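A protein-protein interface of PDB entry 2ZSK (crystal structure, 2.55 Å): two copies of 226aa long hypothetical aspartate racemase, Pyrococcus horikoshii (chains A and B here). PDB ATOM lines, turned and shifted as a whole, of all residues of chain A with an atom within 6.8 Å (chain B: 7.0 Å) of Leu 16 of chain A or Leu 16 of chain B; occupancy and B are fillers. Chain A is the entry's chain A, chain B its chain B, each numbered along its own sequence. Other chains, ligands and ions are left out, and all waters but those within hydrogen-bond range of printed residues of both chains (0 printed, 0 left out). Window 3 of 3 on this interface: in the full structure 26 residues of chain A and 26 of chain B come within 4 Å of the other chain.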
ATOM      1  N   THR A  11      17.719  15.735   1.932  1.00  0.00           N
ATOM      2  CA  THR A  11      18.069  16.280   0.656  1.00  0.00           C
ATOM      3  C   THR A  11      16.760  16.772   0.109  1.00  0.00           C
ATOM      4  O   THR A  11      15.892  16.005  -0.299  1.00  0.00           O
ATOM      5  CB  THR A  11      18.745  15.259  -0.252  1.00  0.00           C
ATOM      6  OG1 THR A  11      20.088  15.054   0.210  1.00  0.00           O
ATOM      7  CG2 THR A  11      18.783  15.760  -1.678  1.00  0.00           C
ATOM      8  N   PRO A  12      16.568  18.085   0.203  1.00  0.00           N
ATOM      9  CA  PRO A  12      15.357  18.727  -0.289  1.00  0.00           C
ATOM     10  C   PRO A  12      15.084  18.366  -1.753  1.00  0.00           C
ATOM     11  O   PRO A  12      13.923  18.242  -2.152  1.00  0.00           O
ATOM     12  CB  PRO A  12      15.659  20.203  -0.070  1.00  0.00           C
ATOM     13  CG  PRO A  12      16.352  20.162   1.263  1.00  0.00           C
ATOM     14  CD  PRO A  12      17.315  18.993   1.095  1.00  0.00           C
ATOM     15  N   GLU A  13      16.145  18.172  -2.538  1.00  0.00           N
ATOM     16  CA  GLU A  13      15.977  17.822  -3.951  1.00  0.00           C
ATOM     17  C   GLU A  13      15.088  16.590  -4.063  1.00  0.00           C
ATOM     18  O   GLU A  13      14.177  16.511  -4.904  1.00  0.00           O
ATOM     19  CB  GLU A  13      17.320  17.522  -4.625  1.00  0.00           C
ATOM     20  CG  GLU A  13      18.344  18.652  -4.581  1.00  0.00           C
ATOM     21  CD  GLU A  13      19.311  18.541  -3.399  1.00  0.00           C
ATOM     22  OE1 GLU A  13      18.978  19.021  -2.288  1.00  0.00           O
ATOM     23  OE2 GLU A  13      20.409  17.959  -3.584  1.00  0.00           O
ATOM     24  N   SER A  14      15.360  15.635  -3.188  1.00  0.00           N
ATOM     25  CA  SER A  14      14.620  14.391  -3.156  1.00  0.00           C
ATOM     26  C   SER A  14      13.170  14.612  -2.738  1.00  0.00           C
ATOM     27  O   SER A  14      12.260  14.031  -3.322  1.00  0.00           O
ATOM     28  CB  SER A  14      15.313  13.418  -2.207  1.00  0.00           C
ATOM     29  OG  SER A  14      14.501  12.295  -1.982  1.00  0.00           O
ATOM     30  N   THR A  15      12.958  15.455  -1.733  1.00  0.00           N
ATOM     31  CA  THR A  15      11.608  15.750  -1.251  1.00  0.00           C
ATOM     32  C   THR A  15      10.858  16.482  -2.362  1.00  0.00           C
ATOM     33  O   THR A  15       9.679  16.231  -2.588  1.00  0.00           O
ATOM     34  CB  THR A  15      11.622  16.658   0.028  1.00  0.00           C
ATOM     35  OG1 THR A  15      12.244  15.963   1.120  1.00  0.00           O
ATOM     36  CG2 THR A  15      10.203  17.045   0.424  1.00  0.00           C
ATOM     37  N   LEU A  16      11.543  17.395  -3.046  1.00  0.00           N
ATOM     38  CA  LEU A  16      10.933  18.155  -4.140  1.00  0.00           C
ATOM     39  C   LEU A  16      10.386  17.206  -5.204  1.00  0.00           C
ATOM     40  O   LEU A  16       9.296  17.404  -5.731  1.00  0.00           O
ATOM     41  CB  LEU A  16      11.963  19.083  -4.787  1.00  0.00           C
ATOM     42  CG  LEU A  16      11.474  20.006  -5.908  1.00  0.00           C
ATOM     43  CD1 LEU A  16      10.586  21.117  -5.328  1.00  0.00           C
ATOM     44  CD2 LEU A  16      12.677  20.625  -6.601  1.00  0.00           C
ATOM     45  N   TYR A  17      11.158  16.170  -5.509  1.00  0.00           N
ATOM     46  CA  TYR A  17      10.772  15.193  -6.507  1.00  0.00           C
ATOM     47  C   TYR A  17       9.547  14.410  -6.055  1.00  0.00           C
ATOM     48  O   TYR A  17       8.642  14.144  -6.851  1.00  0.00           O
ATOM     49  CB  TYR A  17      11.926  14.236  -6.772  1.00  0.00           C
ATOM     50  CG  TYR A  17      11.672  13.318  -7.932  1.00  0.00           C
ATOM     51  CD1 TYR A  17      11.763  13.780  -9.246  1.00  0.00           C
ATOM     52  CD2 TYR A  17      11.291  11.993  -7.719  1.00  0.00           C
ATOM     53  CE1 TYR A  17      11.475  12.942 -10.317  1.00  0.00           C
ATOM     54  CE2 TYR A  17      11.001  11.155  -8.773  1.00  0.00           C
ATOM     55  CZ  TYR A  17      11.092  11.632 -10.073  1.00  0.00           C
ATOM     56  OH  TYR A  17      10.786  10.801 -11.119  1.00  0.00           O
ATOM     57  N   TYR A  18       9.515  14.026  -4.783  1.00  0.00           N
ATOM     58  CA  TYR A  18       8.363  13.288  -4.279  1.00  0.00           C
ATOM     59  C   TYR A  18       7.100  14.097  -4.469  1.00  0.00           C
ATOM     60  O   TYR A  18       6.082  13.574  -4.919  1.00  0.00           O
ATOM     61  CB  TYR A  18       8.517  12.945  -2.790  1.00  0.00           C
ATOM     62  CG  TYR A  18       9.152  11.606  -2.536  1.00  0.00           C
ATOM     63  CD1 TYR A  18      10.504  11.390  -2.820  1.00  0.00           C
ATOM     64  CD2 TYR A  18       8.401  10.541  -2.022  1.00  0.00           C
ATOM     65  CE1 TYR A  18      11.096  10.148  -2.596  1.00  0.00           C
ATOM     66  CE2 TYR A  18       8.985   9.299  -1.798  1.00  0.00           C
ATOM     67  CZ  TYR A  18      10.335   9.107  -2.089  1.00  0.00           C
ATOM     68  OH  TYR A  18      10.925   7.869  -1.894  1.00  0.00           O
ATOM     69  N   TYR A  19       7.161  15.382  -4.136  1.00  0.00           N
ATOM     70  CA  TYR A  19       5.984  16.227  -4.263  1.00  0.00           C
ATOM     71  C   TYR A  19       5.492  16.300  -5.704  1.00  0.00           C
ATOM     72  O   TYR A  19       4.285  16.287  -5.965  1.00  0.00           O
ATOM     73  CB  TYR A  19       6.275  17.630  -3.739  1.00  0.00           C
ATOM     74  CG  TYR A  19       5.018  18.409  -3.410  1.00  0.00           C
ATOM     75  CD1 TYR A  19       4.639  19.503  -4.173  1.00  0.00           C
ATOM     76  CD2 TYR A  19       4.214  18.050  -2.328  1.00  0.00           C
ATOM     77  CE1 TYR A  19       3.496  20.231  -3.869  1.00  0.00           C
ATOM     78  CE2 TYR A  19       3.059  18.771  -2.009  1.00  0.00           C
ATOM     79  CZ  TYR A  19       2.709  19.862  -2.785  1.00  0.00           C
ATOM     80  OH  TYR A  19       1.587  20.597  -2.489  1.00  0.00           O
ATOM     81  N   LYS A  20       6.434  16.379  -6.635  1.00  0.00           N
ATOM     82  CA  LYS A  20       6.103  16.434  -8.047  1.00  0.00           C
ATOM     83  C   LYS A  20       5.363  15.140  -8.424  1.00  0.00           C
ATOM     84  O   LYS A  20       4.297  15.177  -9.045  1.00  0.00           O
ATOM     85  CB  LYS A  20       7.382  16.577  -8.866  1.00  0.00           C
ATOM     86  CG  LYS A  20       7.148  16.874 -10.325  1.00  0.00           C
ATOM     87  CD  LYS A  20       8.464  17.033 -11.065  1.00  0.00           C
ATOM     88  CE  LYS A  20       8.218  17.564 -12.466  1.00  0.00           C
ATOM     89  NZ  LYS A  20       7.580  18.920 -12.416  1.00  0.00           N
ATOM     90  N   LYS A  21       5.921  13.998  -8.031  1.00  0.00           N
ATOM     91  CA  LYS A  21       5.294  12.723  -8.332  1.00  0.00           C
ATOM     92  C   LYS A  21       3.915  12.666  -7.684  1.00  0.00           C
ATOM     93  O   LYS A  21       2.978  12.078  -8.236  1.00  0.00           O
ATOM     94  CB  LYS A  21       6.152  11.569  -7.821  1.00  0.00           C
ATOM     95  CG  LYS A  21       7.550  11.490  -8.396  1.00  0.00           C
ATOM     96  CD  LYS A  21       7.563  11.057  -9.858  1.00  0.00           C
ATOM     97  CE  LYS A  21       7.345  12.220 -10.807  1.00  0.00           C
ATOM     98  NZ  LYS A  21       7.460  11.745 -12.212  1.00  0.00           N
ATOM     99  N   ILE A  23       1.896  15.139  -7.233  1.00  0.00           N
ATOM    100  CA  ILE A  23       0.995  15.927  -8.063  1.00  0.00           C
ATOM    101  C   ILE A  23       0.588  15.113  -9.291  1.00  0.00           C
ATOM    102  O   ILE A  23      -0.602  14.971  -9.580  1.00  0.00           O
ATOM    103  CB  ILE A  23       1.655  17.257  -8.497  1.00  0.00           C
ATOM    104  CG1 ILE A  23       1.879  18.149  -7.269  1.00  0.00           C
ATOM    105  CG2 ILE A  23       0.778  17.978  -9.496  1.00  0.00           C
ATOM    106  CD1 ILE A  23       2.840  19.295  -7.507  1.00  0.00           C
ATOM    107  N   THR B  11      -2.982  24.742  -4.602  1.00  0.00           N
ATOM    108  CA  THR B  11      -2.415  24.473  -5.884  1.00  0.00           C
ATOM    109  C   THR B  11      -1.047  23.968  -5.546  1.00  0.00           C
ATOM    110  O   THR B  11      -0.162  24.712  -5.123  1.00  0.00           O
ATOM    111  CB  THR B  11      -2.403  25.698  -6.802  1.00  0.00           C
ATOM    112  OG1 THR B  11      -3.653  25.733  -7.501  1.00  0.00           O
ATOM    113  CG2 THR B  11      -1.272  25.621  -7.808  1.00  0.00           C
ATOM    114  N   PRO B  12      -0.897  22.647  -5.624  1.00  0.00           N
ATOM    115  CA  PRO B  12       0.389  22.040  -5.327  1.00  0.00           C
ATOM    116  C   PRO B  12       1.443  22.691  -6.202  1.00  0.00           C
ATOM    117  O   PRO B  12       2.581  22.851  -5.776  1.00  0.00           O
ATOM    118  CB  PRO B  12       0.149  20.573  -5.657  1.00  0.00           C
ATOM    119  CG  PRO B  12      -1.276  20.379  -5.207  1.00  0.00           C
ATOM    120  CD  PRO B  12      -1.958  21.628  -5.740  1.00  0.00           C
ATOM    121  N   GLU B  13       1.066  23.081  -7.420  1.00  0.00           N
ATOM    122  CA  GLU B  13       2.022  23.721  -8.329  1.00  0.00           C
ATOM    123  C   GLU B  13       2.686  24.887  -7.632  1.00  0.00           C
ATOM    124  O   GLU B  13       3.908  25.044  -7.669  1.00  0.00           O
ATOM    125  CB  GLU B  13       1.328  24.225  -9.596  1.00  0.00           C
ATOM    126  CG  GLU B  13       1.294  23.200 -10.724  1.00  0.00           C
ATOM    127  CD  GLU B  13       2.243  23.550 -11.870  1.00  0.00           C
ATOM    128  OE1 GLU B  13       3.487  23.601 -11.652  1.00  0.00           O
ATOM    129  OE2 GLU B  13       1.735  23.775 -12.998  1.00  0.00           O
ATOM    130  N   SER B  14       1.863  25.700  -6.987  1.00  0.00           N
ATOM    131  CA  SER B  14       2.363  26.854  -6.269  1.00  0.00           C
ATOM    132  C   SER B  14       3.216  26.461  -5.060  1.00  0.00           C
ATOM    133  O   SER B  14       4.179  27.148  -4.726  1.00  0.00           O
ATOM    134  CB  SER B  14       1.198  27.724  -5.814  1.00  0.00           C
ATOM    135  OG  SER B  14       1.678  28.825  -5.081  1.00  0.00           O
ATOM    136  N   THR B  15       2.863  25.358  -4.409  1.00  0.00           N
ATOM    137  CA  THR B  15       3.603  24.900  -3.246  1.00  0.00           C
ATOM    138  C   THR B  15       4.965  24.366  -3.679  1.00  0.00           C
ATOM    139  O   THR B  15       5.964  24.503  -2.959  1.00  0.00           O
ATOM    140  CB  THR B  15       2.803  23.806  -2.496  1.00  0.00           C
ATOM    141  OG1 THR B  15       1.641  24.397  -1.893  1.00  0.00           O
ATOM    142  CG2 THR B  15       3.655  23.144  -1.423  1.00  0.00           C
ATOM    143  N   LEU B  16       5.004  23.762  -4.864  1.00  0.00           N
ATOM    144  CA  LEU B  16       6.242  23.210  -5.416  1.00  0.00           C
ATOM    145  C   LEU B  16       7.233  24.350  -5.667  1.00  0.00           C
ATOM    146  O   LEU B  16       8.433  24.199  -5.467  1.00  0.00           O
ATOM    147  CB  LEU B  16       5.943  22.486  -6.738  1.00  0.00           C
ATOM    148  CG  LEU B  16       7.081  21.835  -7.535  1.00  0.00           C
ATOM    149  CD1 LEU B  16       7.521  20.537  -6.858  1.00  0.00           C
ATOM    150  CD2 LEU B  16       6.599  21.537  -8.937  1.00  0.00           C
ATOM    151  N   TYR B  17       6.720  25.492  -6.109  1.00  0.00           N
ATOM    152  CA  TYR B  17       7.574  26.633  -6.399  1.00  0.00           C
ATOM    153  C   TYR B  17       8.186  27.157  -5.107  1.00  0.00           C
ATOM    154  O   TYR B  17       9.396  27.407  -5.026  1.00  0.00           O
ATOM    155  CB  TYR B  17       6.760  27.732  -7.077  1.00  0.00           C
ATOM    156  CG  TYR B  17       7.600  28.807  -7.721  1.00  0.00           C
ATOM    157  CD1 TYR B  17       8.191  28.604  -8.970  1.00  0.00           C
ATOM    158  CD2 TYR B  17       7.819  30.026  -7.078  1.00  0.00           C
ATOM    159  CE1 TYR B  17       8.979  29.587  -9.562  1.00  0.00           C
ATOM    160  CE2 TYR B  17       8.606  31.014  -7.662  1.00  0.00           C
ATOM    161  CZ  TYR B  17       9.181  30.784  -8.906  1.00  0.00           C
ATOM    162  OH  TYR B  17       9.951  31.755  -9.479  1.00  0.00           O
ATOM    163  N   TYR B  18       7.340  27.318  -4.092  1.00  0.00           N
ATOM    164  CA  TYR B  18       7.785  27.796  -2.787  1.00  0.00           C
ATOM    165  C   TYR B  18       8.898  26.918  -2.240  1.00  0.00           C
ATOM    166  O   TYR B  18       9.930  27.421  -1.795  1.00  0.00           O
ATOM    167  CB  TYR B  18       6.617  27.810  -1.802  1.00  0.00           C
ATOM    168  CG  TYR B  18       5.886  29.125  -1.738  1.00  0.00           C
ATOM    169  CD1 TYR B  18       5.038  29.541  -2.767  1.00  0.00           C
ATOM    170  CD2 TYR B  18       6.030  29.947  -0.633  1.00  0.00           C
ATOM    171  CE1 TYR B  18       4.344  30.749  -2.679  1.00  0.00           C
ATOM    172  CE2 TYR B  18       5.356  31.142  -0.532  1.00  0.00           C
ATOM    173  CZ  TYR B  18       4.513  31.542  -1.545  1.00  0.00           C
ATOM    174  OH  TYR B  18       3.824  32.721  -1.400  1.00  0.00           O
ATOM    175  N   TYR B  19       8.690  25.604  -2.264  1.00  0.00           N
ATOM    176  CA  TYR B  19       9.711  24.691  -1.763  1.00  0.00           C
ATOM    177  C   TYR B  19      10.958  24.707  -2.641  1.00  0.00           C
ATOM    178  O   TYR B  19      12.059  24.404  -2.178  1.00  0.00           O
ATOM    179  CB  TYR B  19       9.169  23.270  -1.663  1.00  0.00           C
ATOM    180  CG  TYR B  19      10.095  22.335  -0.919  1.00  0.00           C
ATOM    181  CD1 TYR B  19      10.986  21.506  -1.611  1.00  0.00           C
ATOM    182  CD2 TYR B  19      10.079  22.270   0.480  1.00  0.00           C
ATOM    183  CE1 TYR B  19      11.827  20.633  -0.932  1.00  0.00           C
ATOM    184  CE2 TYR B  19      10.921  21.401   1.166  1.00  0.00           C
ATOM    185  CZ  TYR B  19      11.787  20.585   0.458  1.00  0.00           C
ATOM    186  OH  TYR B  19      12.599  19.697   1.128  1.00  0.00           O
ATOM    187  N   LYS B  20      10.792  25.056  -3.911  1.00  0.00           N
ATOM    188  CA  LYS B  20      11.944  25.109  -4.788  1.00  0.00           C
ATOM    189  C   LYS B  20      12.769  26.335  -4.406  1.00  0.00           C
ATOM    190  O   LYS B  20      13.997  26.250  -4.281  1.00  0.00           O
ATOM    191  CB  LYS B  20      11.509  25.184  -6.247  1.00  0.00           C
ATOM    192  CG  LYS B  20      12.660  25.161  -7.229  1.00  0.00           C
ATOM    193  CD  LYS B  20      12.138  25.159  -8.645  1.00  0.00           C
ATOM    194  CE  LYS B  20      13.271  25.135  -9.641  1.00  0.00           C
ATOM    195  NZ  LYS B  20      12.742  25.200 -11.035  1.00  0.00           N
ATOM    196  N   LYS B  21      12.098  27.471  -4.206  1.00  0.00           N
ATOM    197  CA  LYS B  21      12.793  28.693  -3.806  1.00  0.00           C
ATOM    198  C   LYS B  21      13.449  28.480  -2.448  1.00  0.00           C
ATOM    199  O   LYS B  21      14.597  28.872  -2.227  1.00  0.00           O
ATOM    200  CB  LYS B  21      11.826  29.877  -3.762  1.00  0.00           C
ATOM    201  CG  LYS B  21      11.455  30.395  -5.147  1.00  0.00           C
ATOM    202  CD  LYS B  21      12.713  30.741  -5.945  1.00  0.00           C
ATOM    203  CE  LYS B  21      12.395  31.107  -7.378  1.00  0.00           C
ATOM    204  NZ  LYS B  21      13.624  31.506  -8.122  1.00  0.00           N
ATOM    205  N   TYR B  22      12.714  27.850  -1.539  1.00  0.00           N
ATOM    206  CA  TYR B  22      13.226  27.533  -0.210  1.00  0.00           C
ATOM    207  C   TYR B  22      14.629  26.942  -0.380  1.00  0.00           C
ATOM    208  O   TYR B  22      15.583  27.401   0.242  1.00  0.00           O
ATOM    209  CB  TYR B  22      12.282  26.515   0.450  1.00  0.00           C
ATOM    210  CG  TYR B  22      12.848  25.758   1.631  1.00  0.00           C
ATOM    211  CD1 TYR B  22      12.982  26.369   2.891  1.00  0.00           C
ATOM    212  CD2 TYR B  22      13.215  24.414   1.501  1.00  0.00           C
ATOM    213  CE1 TYR B  22      13.459  25.655   3.990  1.00  0.00           C
ATOM    214  CE2 TYR B  22      13.693  23.693   2.585  1.00  0.00           C
ATOM    215  CZ  TYR B  22      13.811  24.315   3.827  1.00  0.00           C
ATOM    216  OH  TYR B  22      14.264  23.581   4.901  1.00  0.00           O
ATOM    217  N   ILE B  23      14.742  25.933  -1.241  1.00  0.00           N
ATOM    218  CA  ILE B  23      16.018  25.272  -1.506  1.00  0.00           C
ATOM    219  C   ILE B  23      17.034  26.248  -2.080  1.00  0.00           C
ATOM    220  O   ILE B  23      18.145  26.369  -1.568  1.00  0.00           O
ATOM    221  CB  ILE B  23      15.840  24.108  -2.495  1.00  0.00           C
ATOM    222  CG1 ILE B  23      14.940  23.038  -1.861  1.00  0.00           C
ATOM    223  CG2 ILE B  23      17.203  23.552  -2.907  1.00  0.00           C
ATOM    224  CD1 ILE B  23      14.515  21.922  -2.805  1.00  0.00           C
ATOM    225  N   ALA B  80       1.023  29.437   1.029  1.00  0.00           N
ATOM    226  CA  ALA B  80       1.862  29.261  -0.151  1.00  0.00           C
ATOM    227  C   ALA B  80       1.019  29.583  -1.387  1.00  0.00           C
ATOM    228  O   ALA B  80       0.893  28.762  -2.298  1.00  0.00           O
ATOM    229  CB  ALA B  80       2.389  27.830  -0.220  1.00  0.00           C
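OH of Tyr 19 of chain B touches CA of Pro 12 of chain A, 3.2 Å away.
Ile 23 of chain B touches Pro 12 of chain A.
OH of Tyr 19 of chain B touches CB of Thr 15 of chain A (3.4 Å).
Leu 16 of chain A touches Leu 16 of chain B.
CD1 of Leu 16 of chain A touches CD1 of Tyr 19 of chain B, at 3.8 Å.
Tyr 19 of chain A touches Pro 12 of chain B (CE1 to O, 3.4 Å).
Tyr 19 of chain A touches Thr 15 of chain B (OH to CB, 3.4 Å).
Tyr 19 of chain A touches Leu 16 of chain B (CE1 to N, 3.97 Å).
CB of Pro 12 of chain B touches CG1 of Ile 23 of chain A, 3.4 Å away.
Of chain B, only Leu 16 (3.5 Å) and Tyr 19 (3.8 Å) come within 4 Å of Leu 16 of chain A.
Of the printed residues of chain A, Ile 23 of chain B touches Pro 12 (3.4 Å).
Of the printed residues of chain B, Tyr 19 of chain A touches Pro 12 (3.4 Å), Thr 15 (3.4 Å) and Leu 16 (3.97 Å).
Printed residues of chain B within 4 Å of Pro 12 of chain A: Tyr 19 (3.2 Å) and Ile 23 (3.4 Å).
Of the printed residues of chain B, Ile 23 of chain A touches Pro 12.
Of the printed residues of chain A, Tyr 19 of chain B touches Pro 12, Thr 15 and Leu 16.
The nearest residue of chain B that does not touch Leu 16 of chain A is Lys 20 of chain B (4.2 Å).
Of the 12 printed residues of chain A, 5 touch a printed residue of chain B.
Hydrophobic or aromatic side chains of chain A within 4 Å of the printed part of chain B: Pro 12, Leu 16, Tyr 19 and Ile 23.
Among the printed residues, no Asp or Glu carboxylate lies within 4 Å of a Lys or Arg side-chain nitrogen of the other chain.
Pro 12 of chain A touches Ile 23 of chain B, and with the chains exchanged Ile 23 of chain A touches Pro 12 of chain B.
Thr 15 of chain A touches Tyr 19 of chain B, and with the chains exchanged Tyr 19 of chain A touches Thr 15 of chain B.
Leu 16 of chain A touches its own counterpart, Leu 16 of chain B.
Leu 16 of chain A touches Tyr 19 of chain B, and with the chains exchanged Tyr 19 of chain A touches Leu 16 of chain B.
12 positions are printed for both chains.
Of the 9 pairs that touch across the chains among the printed residues, 9 have their exchanged pair printed and touching as well.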
